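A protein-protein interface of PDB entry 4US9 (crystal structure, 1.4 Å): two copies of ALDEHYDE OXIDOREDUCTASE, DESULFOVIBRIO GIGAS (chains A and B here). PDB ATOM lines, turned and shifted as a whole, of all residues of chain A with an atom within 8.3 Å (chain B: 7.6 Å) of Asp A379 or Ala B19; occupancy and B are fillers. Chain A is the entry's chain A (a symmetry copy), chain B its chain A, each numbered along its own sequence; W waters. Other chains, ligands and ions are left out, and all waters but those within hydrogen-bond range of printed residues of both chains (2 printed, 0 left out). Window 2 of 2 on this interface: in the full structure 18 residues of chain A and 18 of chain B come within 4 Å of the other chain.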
ATOM      1  N   PRO A 204     -14.224  19.917  21.158  1.00  0.00           N
ATOM      2  CA  PRO A 204     -13.928  19.894  19.727  1.00  0.00           C
ATOM      3  C   PRO A 204     -13.601  21.229  19.128  1.00  0.00           C
ATOM      4  O   PRO A 204     -13.950  22.261  19.682  1.00  0.00           O
ATOM      5  CB  PRO A 204     -15.193  19.348  19.107  1.00  0.00           C
ATOM      6  CG  PRO A 204     -16.267  19.543  20.053  1.00  0.00           C
ATOM      7  CD  PRO A 204     -15.638  19.699  21.441  1.00  0.00           C
ATOM      8  N   TYR A 376     -23.388  24.383  26.017  1.00  0.00           N
ATOM      9  CA  TYR A 376     -23.642  24.008  24.643  1.00  0.00           C
ATOM     10  C   TYR A 376     -25.123  23.745  24.489  1.00  0.00           C
ATOM     11  O   TYR A 376     -25.835  23.495  25.449  1.00  0.00           O
ATOM     12  CB  TYR A 376     -22.810  22.757  24.238  1.00  0.00           C
ATOM     13  CG  TYR A 376     -22.977  21.571  25.160  1.00  0.00           C
ATOM     14  CD1 TYR A 376     -23.967  20.629  24.941  1.00  0.00           C
ATOM     15  CD2 TYR A 376     -22.149  21.401  26.273  1.00  0.00           C
ATOM     16  CE1 TYR A 376     -24.142  19.560  25.816  1.00  0.00           C
ATOM     17  CE2 TYR A 376     -22.321  20.342  27.138  1.00  0.00           C
ATOM     18  CZ  TYR A 376     -23.345  19.445  26.936  1.00  0.00           C
ATOM     19  OH  TYR A 376     -23.536  18.404  27.800  1.00  0.00           O
ATOM     20  N   MET A 377     -25.578  23.764  23.240  1.00  0.00           N
ATOM     21  CA  MET A 377     -26.931  23.337  22.912  1.00  0.00           C
ATOM     22  C   MET A 377     -26.886  21.850  22.599  1.00  0.00           C
ATOM     23  O   MET A 377     -26.117  21.390  21.742  1.00  0.00           O
ATOM     24  CB  MET A 377     -27.486  24.115  21.729  1.00  0.00           C
ATOM     25  CG  MET A 377     -27.452  25.618  21.926  1.00  0.00           C
ATOM     26  SD  MET A 377     -28.210  26.220  23.458  1.00  0.00           S
ATOM     27  CE  MET A 377     -29.883  25.692  23.249  1.00  0.00           C
ATOM     28  N   GLY A 378     -27.662  21.087  23.352  1.00  0.00           N
ATOM     29  CA  GLY A 378     -27.732  19.653  23.165  1.00  0.00           C
ATOM     30  C   GLY A 378     -28.500  19.292  21.920  1.00  0.00           C
ATOM     31  O   GLY A 378     -29.252  20.101  21.356  1.00  0.00           O
ATOM     32  N   ASP A 379     -28.355  18.046  21.494  1.00  0.00           N
ATOM     33  CA  ASP A 379     -29.085  17.595  20.302  1.00  0.00           C
ATOM     34  C   ASP A 379     -30.594  17.458  20.596  1.00  0.00           C
ATOM     35  O   ASP A 379     -31.430  17.453  19.691  1.00  0.00           O
ATOM     36  CB  ASP A 379     -28.431  16.262  19.854  1.00  0.00           C
ATOM     37  CG  ASP A 379     -26.886  16.374  19.646  1.00  0.00           C
ATOM     38  OD1 ASP A 379     -26.413  17.509  19.386  1.00  0.00           O
ATOM     39  OD2 ASP A 379     -26.143  15.337  19.740  1.00  0.00           O
ATOM     40  N   ASP A 380     -30.919  17.404  21.888  1.00  0.00           N
ATOM     41  CA  ASP A 380     -32.292  17.395  22.394  1.00  0.00           C
ATOM     42  C   ASP A 380     -32.961  18.777  22.496  1.00  0.00           C
ATOM     43  O   ASP A 380     -34.098  18.880  22.979  1.00  0.00           O
ATOM     44  CB  ASP A 380     -32.297  16.722  23.773  1.00  0.00           C
ATOM     45  CG  ASP A 380     -31.476  17.468  24.802  1.00  0.00           C
ATOM     46  OD1 ASP A 380     -30.921  18.547  24.486  1.00  0.00           O
ATOM     47  OD2 ASP A 380     -31.407  16.950  25.929  1.00  0.00           O
ATOM     48  N   GLY A 381     -32.247  19.829  22.091  1.00  0.00           N
ATOM     49  CA  GLY A 381     -32.751  21.208  22.129  1.00  0.00           C
ATOM     50  C   GLY A 381     -32.520  21.959  23.444  1.00  0.00           C
ATOM     51  O   GLY A 381     -32.772  23.167  23.527  1.00  0.00           O
ATOM     52  N   LYS A 382     -32.048  21.258  24.471  1.00  0.00           N
ATOM     53  CA  LYS A 382     -31.810  21.892  25.763  1.00  0.00           C
ATOM     54  C   LYS A 382     -30.450  22.589  25.806  1.00  0.00           C
ATOM     55  O   LYS A 382     -29.546  22.242  25.048  1.00  0.00           O
ATOM     56  CB  LYS A 382     -31.892  20.867  26.888  1.00  0.00           C
ATOM     57  CG  LYS A 382     -33.231  20.140  26.938  1.00  0.00           C
ATOM     58  CD  LYS A 382     -33.325  19.215  28.143  1.00  0.00           C
ATOM     59  CE  LYS A 382     -34.641  18.439  28.155  1.00  0.00           C
ATOM     60  NZ  LYS A 382     -34.800  17.693  29.428  1.00  0.00           N
ATOM     61  N   CYS A 383     -30.312  23.575  26.694  1.00  0.00           N
ATOM     62  CA  CYS A 383     -29.033  24.216  26.946  1.00  0.00           C
ATOM     63  C   CYS A 383     -28.397  23.544  28.154  1.00  0.00           C
ATOM     64  O   CYS A 383     -29.008  23.479  29.212  1.00  0.00           O
ATOM     65  CB  CYS A 383     -29.234  25.702  27.208  1.00  0.00           C
ATOM     66  SG  CYS A 383     -27.696  26.609  27.512  1.00  0.00           S
ATOM     67  N   TYR A 384     -27.181  23.029  27.962  1.00  0.00           N
ATOM     68  CA  TYR A 384     -26.409  22.358  29.018  1.00  0.00           C
ATOM     69  C   TYR A 384     -25.298  23.269  29.497  1.00  0.00           C
ATOM     70  O   TYR A 384     -24.556  23.833  28.680  1.00  0.00           O
ATOM     71  CB  TYR A 384     -25.774  21.057  28.506  1.00  0.00           C
ATOM     72  CG  TYR A 384     -26.761  19.949  28.260  1.00  0.00           C
ATOM     73  CD1 TYR A 384     -27.614  19.976  27.143  1.00  0.00           C
ATOM     74  CD2 TYR A 384     -26.879  18.902  29.148  1.00  0.00           C
ATOM     75  CE1 TYR A 384     -28.554  18.977  26.934  1.00  0.00           C
ATOM     76  CE2 TYR A 384     -27.817  17.901  28.948  1.00  0.00           C
ATOM     77  CZ  TYR A 384     -28.644  17.938  27.835  1.00  0.00           C
ATOM     78  OH  TYR A 384     -29.579  16.947  27.658  1.00  0.00           O
ATOM     79  N   MET B   1     -24.254  19.203  20.512  1.00  0.00           N
ATOM     80  CA  MET B   1     -23.102  18.526  21.197  1.00  0.00           C
ATOM     81  C   MET B   1     -23.726  17.590  22.197  1.00  0.00           C
ATOM     82  O   MET B   1     -24.854  17.814  22.657  1.00  0.00           O
ATOM     83  CB  MET B   1     -22.233  19.594  21.894  1.00  0.00           C
ATOM     84  CG  MET B   1     -21.295  19.075  22.999  1.00  0.00           C
ATOM     85  SD  MET B   1     -20.094  20.317  23.501  1.00  0.00           S
ATOM     86  CE  MET B   1     -18.822  20.132  22.273  1.00  0.00           C
ATOM     87  N   ILE B   2     -22.983  16.557  22.578  1.00  0.00           N
ATOM     88  CA  ILE B   2     -23.439  15.627  23.608  1.00  0.00           C
ATOM     89  C   ILE B   2     -22.258  15.245  24.523  1.00  0.00           C
ATOM     90  O   ILE B   2     -21.113  15.133  24.078  1.00  0.00           O
ATOM     91  CB  ILE B   2     -24.157  14.395  23.013  1.00  0.00           C
ATOM     92  CG1 ILE B   2     -24.917  13.612  24.103  1.00  0.00           C
ATOM     93  CG2 ILE B   2     -23.194  13.553  22.186  1.00  0.00           C
ATOM     94  CD1 ILE B   2     -26.063  12.806  23.538  1.00  0.00           C
ATOM     95  N   GLN B   3     -22.582  15.058  25.794  1.00  0.00           N
ATOM     96  CA  GLN B   3     -21.669  14.460  26.766  1.00  0.00           C
ATOM     97  C   GLN B   3     -21.761  12.939  26.665  1.00  0.00           C
ATOM     98  O   GLN B   3     -22.867  12.391  26.661  1.00  0.00           O
ATOM     99  CB  GLN B   3     -22.081  14.886  28.175  1.00  0.00           C
ATOM    100  CG  GLN B   3     -21.221  14.282  29.291  1.00  0.00           C
ATOM    101  CD  GLN B   3     -21.706  14.642  30.689  1.00  0.00           C
ATOM    102  OE1 GLN B   3     -22.909  14.870  30.899  1.00  0.00           O
ATOM    103  NE2 GLN B   3     -20.820  14.659  31.638  1.00  0.00           N
ATOM    104  N   LYS B   4     -20.611  12.269  26.610  1.00  0.00           N
ATOM    105  CA  LYS B   4     -20.556  10.809  26.624  1.00  0.00           C
ATOM    106  C   LYS B   4     -19.477  10.411  27.618  1.00  0.00           C
ATOM    107  O   LYS B   4     -18.289  10.745  27.428  1.00  0.00           O
ATOM    108  CB  LYS B   4     -20.203  10.261  25.266  1.00  0.00           C
ATOM    109  CG  LYS B   4     -21.286  10.372  24.242  1.00  0.00           C
ATOM    110  CD  LYS B   4     -20.797   9.683  22.984  1.00  0.00           C
ATOM    111  CE  LYS B   4     -21.813   9.855  21.890  1.00  0.00           C
ATOM    112  NZ  LYS B   4     -22.987   8.972  22.096  1.00  0.00           N
ATOM    113  N   PHE B  16     -16.905  15.375  25.477  1.00  0.00           N
ATOM    114  CA  PHE B  16     -17.843  16.311  24.870  1.00  0.00           C
ATOM    115  C   PHE B  16     -17.583  16.330  23.372  1.00  0.00           C
ATOM    116  O   PHE B  16     -16.490  16.724  22.932  1.00  0.00           O
ATOM    117  CB  PHE B  16     -17.680  17.674  25.509  1.00  0.00           C
ATOM    118  CG  PHE B  16     -18.102  17.633  26.954  1.00  0.00           C
ATOM    119  CD1 PHE B  16     -19.427  17.835  27.312  1.00  0.00           C
ATOM    120  CD2 PHE B  16     -17.198  17.287  27.938  1.00  0.00           C
ATOM    121  CE1 PHE B  16     -19.835  17.712  28.619  1.00  0.00           C
ATOM    122  CE2 PHE B  16     -17.602  17.140  29.246  1.00  0.00           C
ATOM    123  CZ  PHE B  16     -18.919  17.367  29.593  1.00  0.00           C
ATOM    124  N   VAL B  17     -18.574  15.854  22.619  1.00  0.00           N
ATOM    125  CA  VAL B  17     -18.394  15.587  21.206  1.00  0.00           C
ATOM    126  C   VAL B  17     -19.601  15.995  20.391  1.00  0.00           C
ATOM    127  O   VAL B  17     -20.720  16.088  20.889  1.00  0.00           O
ATOM    128  CB  VAL B  17     -18.066  14.103  20.921  1.00  0.00           C
ATOM    129  CG1 VAL B  17     -16.719  13.719  21.525  1.00  0.00           C
ATOM    130  CG2 VAL B  17     -19.188  13.198  21.409  1.00  0.00           C
ATOM    131  N   ASP B  18     -19.332  16.198  19.103  1.00  0.00           N
ATOM    132  CA  ASP B  18     -20.384  16.240  18.092  1.00  0.00           C
ATOM    133  C   ASP B  18     -20.725  14.790  17.755  1.00  0.00           C
ATOM    134  O   ASP B  18     -19.838  13.981  17.479  1.00  0.00           O
ATOM    135  CB  ASP B  18     -19.815  16.984  16.864  1.00  0.00           C
ATOM    136  CG  ASP B  18     -20.747  17.020  15.656  1.00  0.00           C
ATOM    137  OD1 ASP B  18     -21.846  16.436  15.692  1.00  0.00           O
ATOM    138  OD2 ASP B  18     -20.344  17.671  14.660  1.00  0.00           O
ATOM    139  N   ALA B  19     -22.015  14.456  17.740  1.00  0.00           N
ATOM    140  CA  ALA B  19     -22.449  13.117  17.415  1.00  0.00           C
ATOM    141  C   ALA B  19     -22.034  12.662  16.008  1.00  0.00           C
ATOM    142  O   ALA B  19     -21.902  11.465  15.762  1.00  0.00           O
ATOM    143  CB  ALA B  19     -23.956  13.007  17.575  1.00  0.00           C
ATOM    144  N   GLU B  20     -21.838  13.617  15.102  1.00  0.00           N
ATOM    145  CA  GLU B  20     -21.392  13.318  13.753  1.00  0.00           C
ATOM    146  C   GLU B  20     -19.878  13.256  13.597  1.00  0.00           C
ATOM    147  O   GLU B  20     -19.398  12.862  12.551  1.00  0.00           O
ATOM    148  CB  GLU B  20     -21.925  14.367  12.772  1.00  0.00           C
ATOM    149  CG  GLU B  20     -23.426  14.323  12.597  1.00  0.00           C
ATOM    150  CD  GLU B  20     -23.845  13.040  11.892  1.00  0.00           C
ATOM    151  OE1 GLU B  20     -23.382  12.808  10.743  1.00  0.00           O
ATOM    152  OE2 GLU B  20     -24.593  12.269  12.496  1.00  0.00           O
ATOM    153  N   ALA B  21     -19.126  13.606  14.636  1.00  0.00           N
ATOM    154  CA  ALA B  21     -17.668  13.580  14.536  1.00  0.00           C
ATOM    155  C   ALA B  21     -17.172  12.157  14.384  1.00  0.00           C
ATOM    156  O   ALA B  21     -17.771  11.207  14.895  1.00  0.00           O
ATOM    157  CB  ALA B  21     -17.025  14.218  15.749  1.00  0.00           C
ATOM    158  N   LEU B  22     -16.036  12.029  13.705  1.00  0.00           N
ATOM    159  CA  LEU B  22     -15.388  10.739  13.528  1.00  0.00           C
ATOM    160  C   LEU B  22     -14.588  10.387  14.778  1.00  0.00           C
ATOM    161  O   LEU B  22     -13.851  11.225  15.325  1.00  0.00           O
ATOM    162  CB  LEU B  22     -14.482  10.742  12.290  1.00  0.00           C
ATOM    163  CG  LEU B  22     -15.186  11.064  10.982  1.00  0.00           C
ATOM    164  CD1 LEU B  22     -14.158  11.205   9.869  1.00  0.00           C
ATOM    165  CD2 LEU B  22     -16.255  10.025  10.671  1.00  0.00           C
ATOM    166  N   THR B  62     -16.234   5.537  11.908  1.00  0.00           N
ATOM    167  CA  THR B  62     -17.124   5.322  13.052  1.00  0.00           C
ATOM    168  C   THR B  62     -17.488   6.688  13.642  1.00  0.00           C
ATOM    169  O   THR B  62     -16.627   7.378  14.205  1.00  0.00           O
ATOM    170  CB  THR B  62     -16.436   4.481  14.134  1.00  0.00           C
ATOM    171  OG1 THR B  62     -15.998   3.240  13.565  1.00  0.00           O
ATOM    172  CG2 THR B  62     -17.363   4.201  15.308  1.00  0.00           C
ATOM    173  N   LYS B  63     -18.746   7.087  13.521  1.00  0.00           N
ATOM    174  CA  LYS B  63     -19.182   8.361  14.093  1.00  0.00           C
ATOM    175  C   LYS B  63     -19.488   8.198  15.573  1.00  0.00           C
ATOM    176  O   LYS B  63     -19.845   7.115  16.035  1.00  0.00           O
ATOM    177  CB  LYS B  63     -20.394   8.918  13.328  1.00  0.00           C
ATOM    178  CG  LYS B  63     -20.027   9.411  11.932  1.00  0.00           C
ATOM    179  CD  LYS B  63     -21.217   9.883  11.137  1.00  0.00           C
ATOM    180  CE  LYS B  63     -20.812  10.397   9.771  1.00  0.00           C
ATOM    181  NZ  LYS B  63     -22.023  10.802   9.004  1.00  0.00           N
ATOM    182  N   MET B  64     -19.382   9.303  16.314  1.00  0.00           N
ATOM    183  CA  MET B  64     -19.584   9.257  17.764  1.00  0.00           C
ATOM    184  C   MET B  64     -20.973   8.808  18.177  1.00  0.00           C
ATOM    185  O   MET B  64     -21.148   8.241  19.261  1.00  0.00           O
ATOM    186  CB  MET B  64     -19.203  10.571  18.424  1.00  0.00           C
ATOM    187  CG  MET B  64     -17.723  10.918  18.348  1.00  0.00           C
ATOM    188  SD  MET B  64     -16.604   9.629  18.940  1.00  0.00           S
ATOM    189  CE  MET B  64     -17.144   9.450  20.631  1.00  0.00           C
ATOM    190  N   LYS B  65     -21.968   9.015  17.320  1.00  0.00           N
ATOM    191  CA  LYS B  65     -23.309   8.509  17.619  1.00  0.00           C
ATOM    192  C   LYS B  65     -23.364   6.987  17.773  1.00  0.00           C
ATOM    193  O   LYS B  65     -24.308   6.453  18.362  1.00  0.00           O
ATOM    194  CB  LYS B  65     -24.285   8.951  16.537  1.00  0.00           C
ATOM    195  CG  LYS B  65     -24.022   8.417  15.149  1.00  0.00           C
ATOM    196  CD  LYS B  65     -24.884   9.188  14.169  1.00  0.00           C
ATOM    197  CE  LYS B  65     -24.540   8.834  12.764  1.00  0.00           C
ATOM    198  NZ  LYS B  65     -25.296   9.733  11.864  1.00  0.00           N
ATOM    199  N   ARG B  66     -22.353   6.292  17.261  1.00  0.00           N
ATOM    200  CA  ARG B  66     -22.254   4.834  17.407  1.00  0.00           C
ATOM    201  C   ARG B  66     -21.514   4.370  18.657  1.00  0.00           C
ATOM    202  O   ARG B  66     -21.392   3.165  18.897  1.00  0.00           O
ATOM    203  CB  ARG B  66     -21.605   4.227  16.148  1.00  0.00           C
ATOM    204  CG  ARG B  66     -22.325   4.611  14.845  1.00  0.00           C
ATOM    205  CD  ARG B  66     -23.806   4.186  14.752  1.00  0.00           C
ATOM    206  NE  ARG B  66     -24.475   4.664  13.517  1.00  0.00           N
ATOM    207  CZ  ARG B  66     -25.667   5.279  13.438  1.00  0.00           C
ATOM    208  NH1 ARG B  66     -26.427   5.535  14.515  1.00  0.00           N
ATOM    209  NH2 ARG B  66     -26.116   5.645  12.236  1.00  0.00           N
ATOM    210  N   VAL B  67     -21.045   5.324  19.461  1.00  0.00           N
ATOM    211  CA  VAL B  67     -20.342   5.034  20.689  1.00  0.00           C
ATOM    212  C   VAL B  67     -21.322   5.304  21.822  1.00  0.00           C
ATOM    213  O   VAL B  67     -21.701   6.437  22.080  1.00  0.00           O
ATOM    214  CB  VAL B  67     -19.086   5.909  20.840  1.00  0.00           C
ATOM    215  CG1 VAL B  67     -18.353   5.561  22.124  1.00  0.00           C
ATOM    216  CG2 VAL B  67     -18.153   5.715  19.634  1.00  0.00           C
HETATM  217  O   HOH W   1     -23.975  16.546  18.537  1.00  0.00           O
HETATM  218  O   HOH W   2     -25.091  16.225  27.070  1.00  0.00           O
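The backbone NH (N) of Met B1 is in hydrogen-bond range of the side-chain carboxylate (OD1) of Asp A379 (3.0 Å). The backbone NH of Met B1 is in hydrogen-bond range of the backbone carbonyl oxygen of Met A377 (3.1 Å).
The backbone NH of Tyr A384 lies within hydrogen-bond range of the backbone carbonyl oxygen of Tyr A376 (2.9 Å). N of Lys B65 lies within hydrogen-bond range of O of Ala B19 (2.9 Å). The backbone NH of Ile B2 lies within hydrogen-bond range of the backbone carbonyl oxygen of Val B17, at 2.9 Å. O of Ala B19 is in hydrogen-bond range of N of Met B64, at 3.4 Å.
Among the printed residues, merely in contact across the chains: Pro A204 with Met B1 (3.3 Å), Pro A204 with Phe B16 (3.4 Å), Gly A378 with Met B1 (3.5 Å), Tyr A376 with Met B1 (3.6 Å), Tyr A376 with Gln B3 (3.8 Å), Tyr A376 with Phe B16 (3.8 Å), Asp A379 with Ala B19 (3.9 Å) and Asp A379 with Ile B2 (3.9 Å).
Of the printed residues of chain B, Pro A204 touches Met B1 and Phe B16. Of the printed residues of chain B, Tyr A376 touches Met B1 (3.6 Å), Gln B3 (3.8 Å) and Phe B16 (3.8 Å). Printed residues of chain B within 4 Å of Gly A378: Met B1 (3.5 Å). Printed residues of chain B within 4 Å of Asp A379: Met B1 (3.0 Å), Ile B2 (3.9 Å) and Ala B19 (3.9 Å). Lys A382 touches none of the printed residues of chain B. Of the printed residues of chain A, Ala B19 touches Asp A379. Lys B65 touches none of the printed residues of chain A. The nearest printed residue of chain B that does not touch Asp A379 is Val B17 (5.6 Å). The nearest printed residue of chain A that does not touch Ala B19 is Pro A204 (8.0 Å). The nearest printed residue of chain B that does not touch Met A377 is Ile B2 (5.8 Å).
Of the 10 printed residues of chain A, 5 touch a printed residue of chain B. Hydrophobic or aromatic side chains of chain A within 4 Å of the printed part of chain B: Pro A204 and Tyr A376. Hydrophobic or aromatic side chains of chain B that line the printed part of chain A: Met B1, Ile B2, Phe B16 and Ala B19. Among the printed residues, 10 pairs touch across the chains. Among the printed residues, no Asp or Glu carboxylate lies within 4 Å of a Lys or Arg side-chain nitrogen of the other chain.
No position is printed for both chains. Of the 10 pairs that touch across the chains among the printed residues, none has its exchanged pair printed and touching as well.
Water W1 lies within hydrogen-bond range of the side-chain carboxylate of Asp A379 (2.8 Å), the backbone NH of Ala B19 (3.0 Å) and the backbone NH of Met B1 (3.3 Å). Water W2 lies within hydrogen-bond range of the side-chain hydroxyl of Tyr A376 (2.8 Å) and the backbone NH of Gln B3 (3.0 Å).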
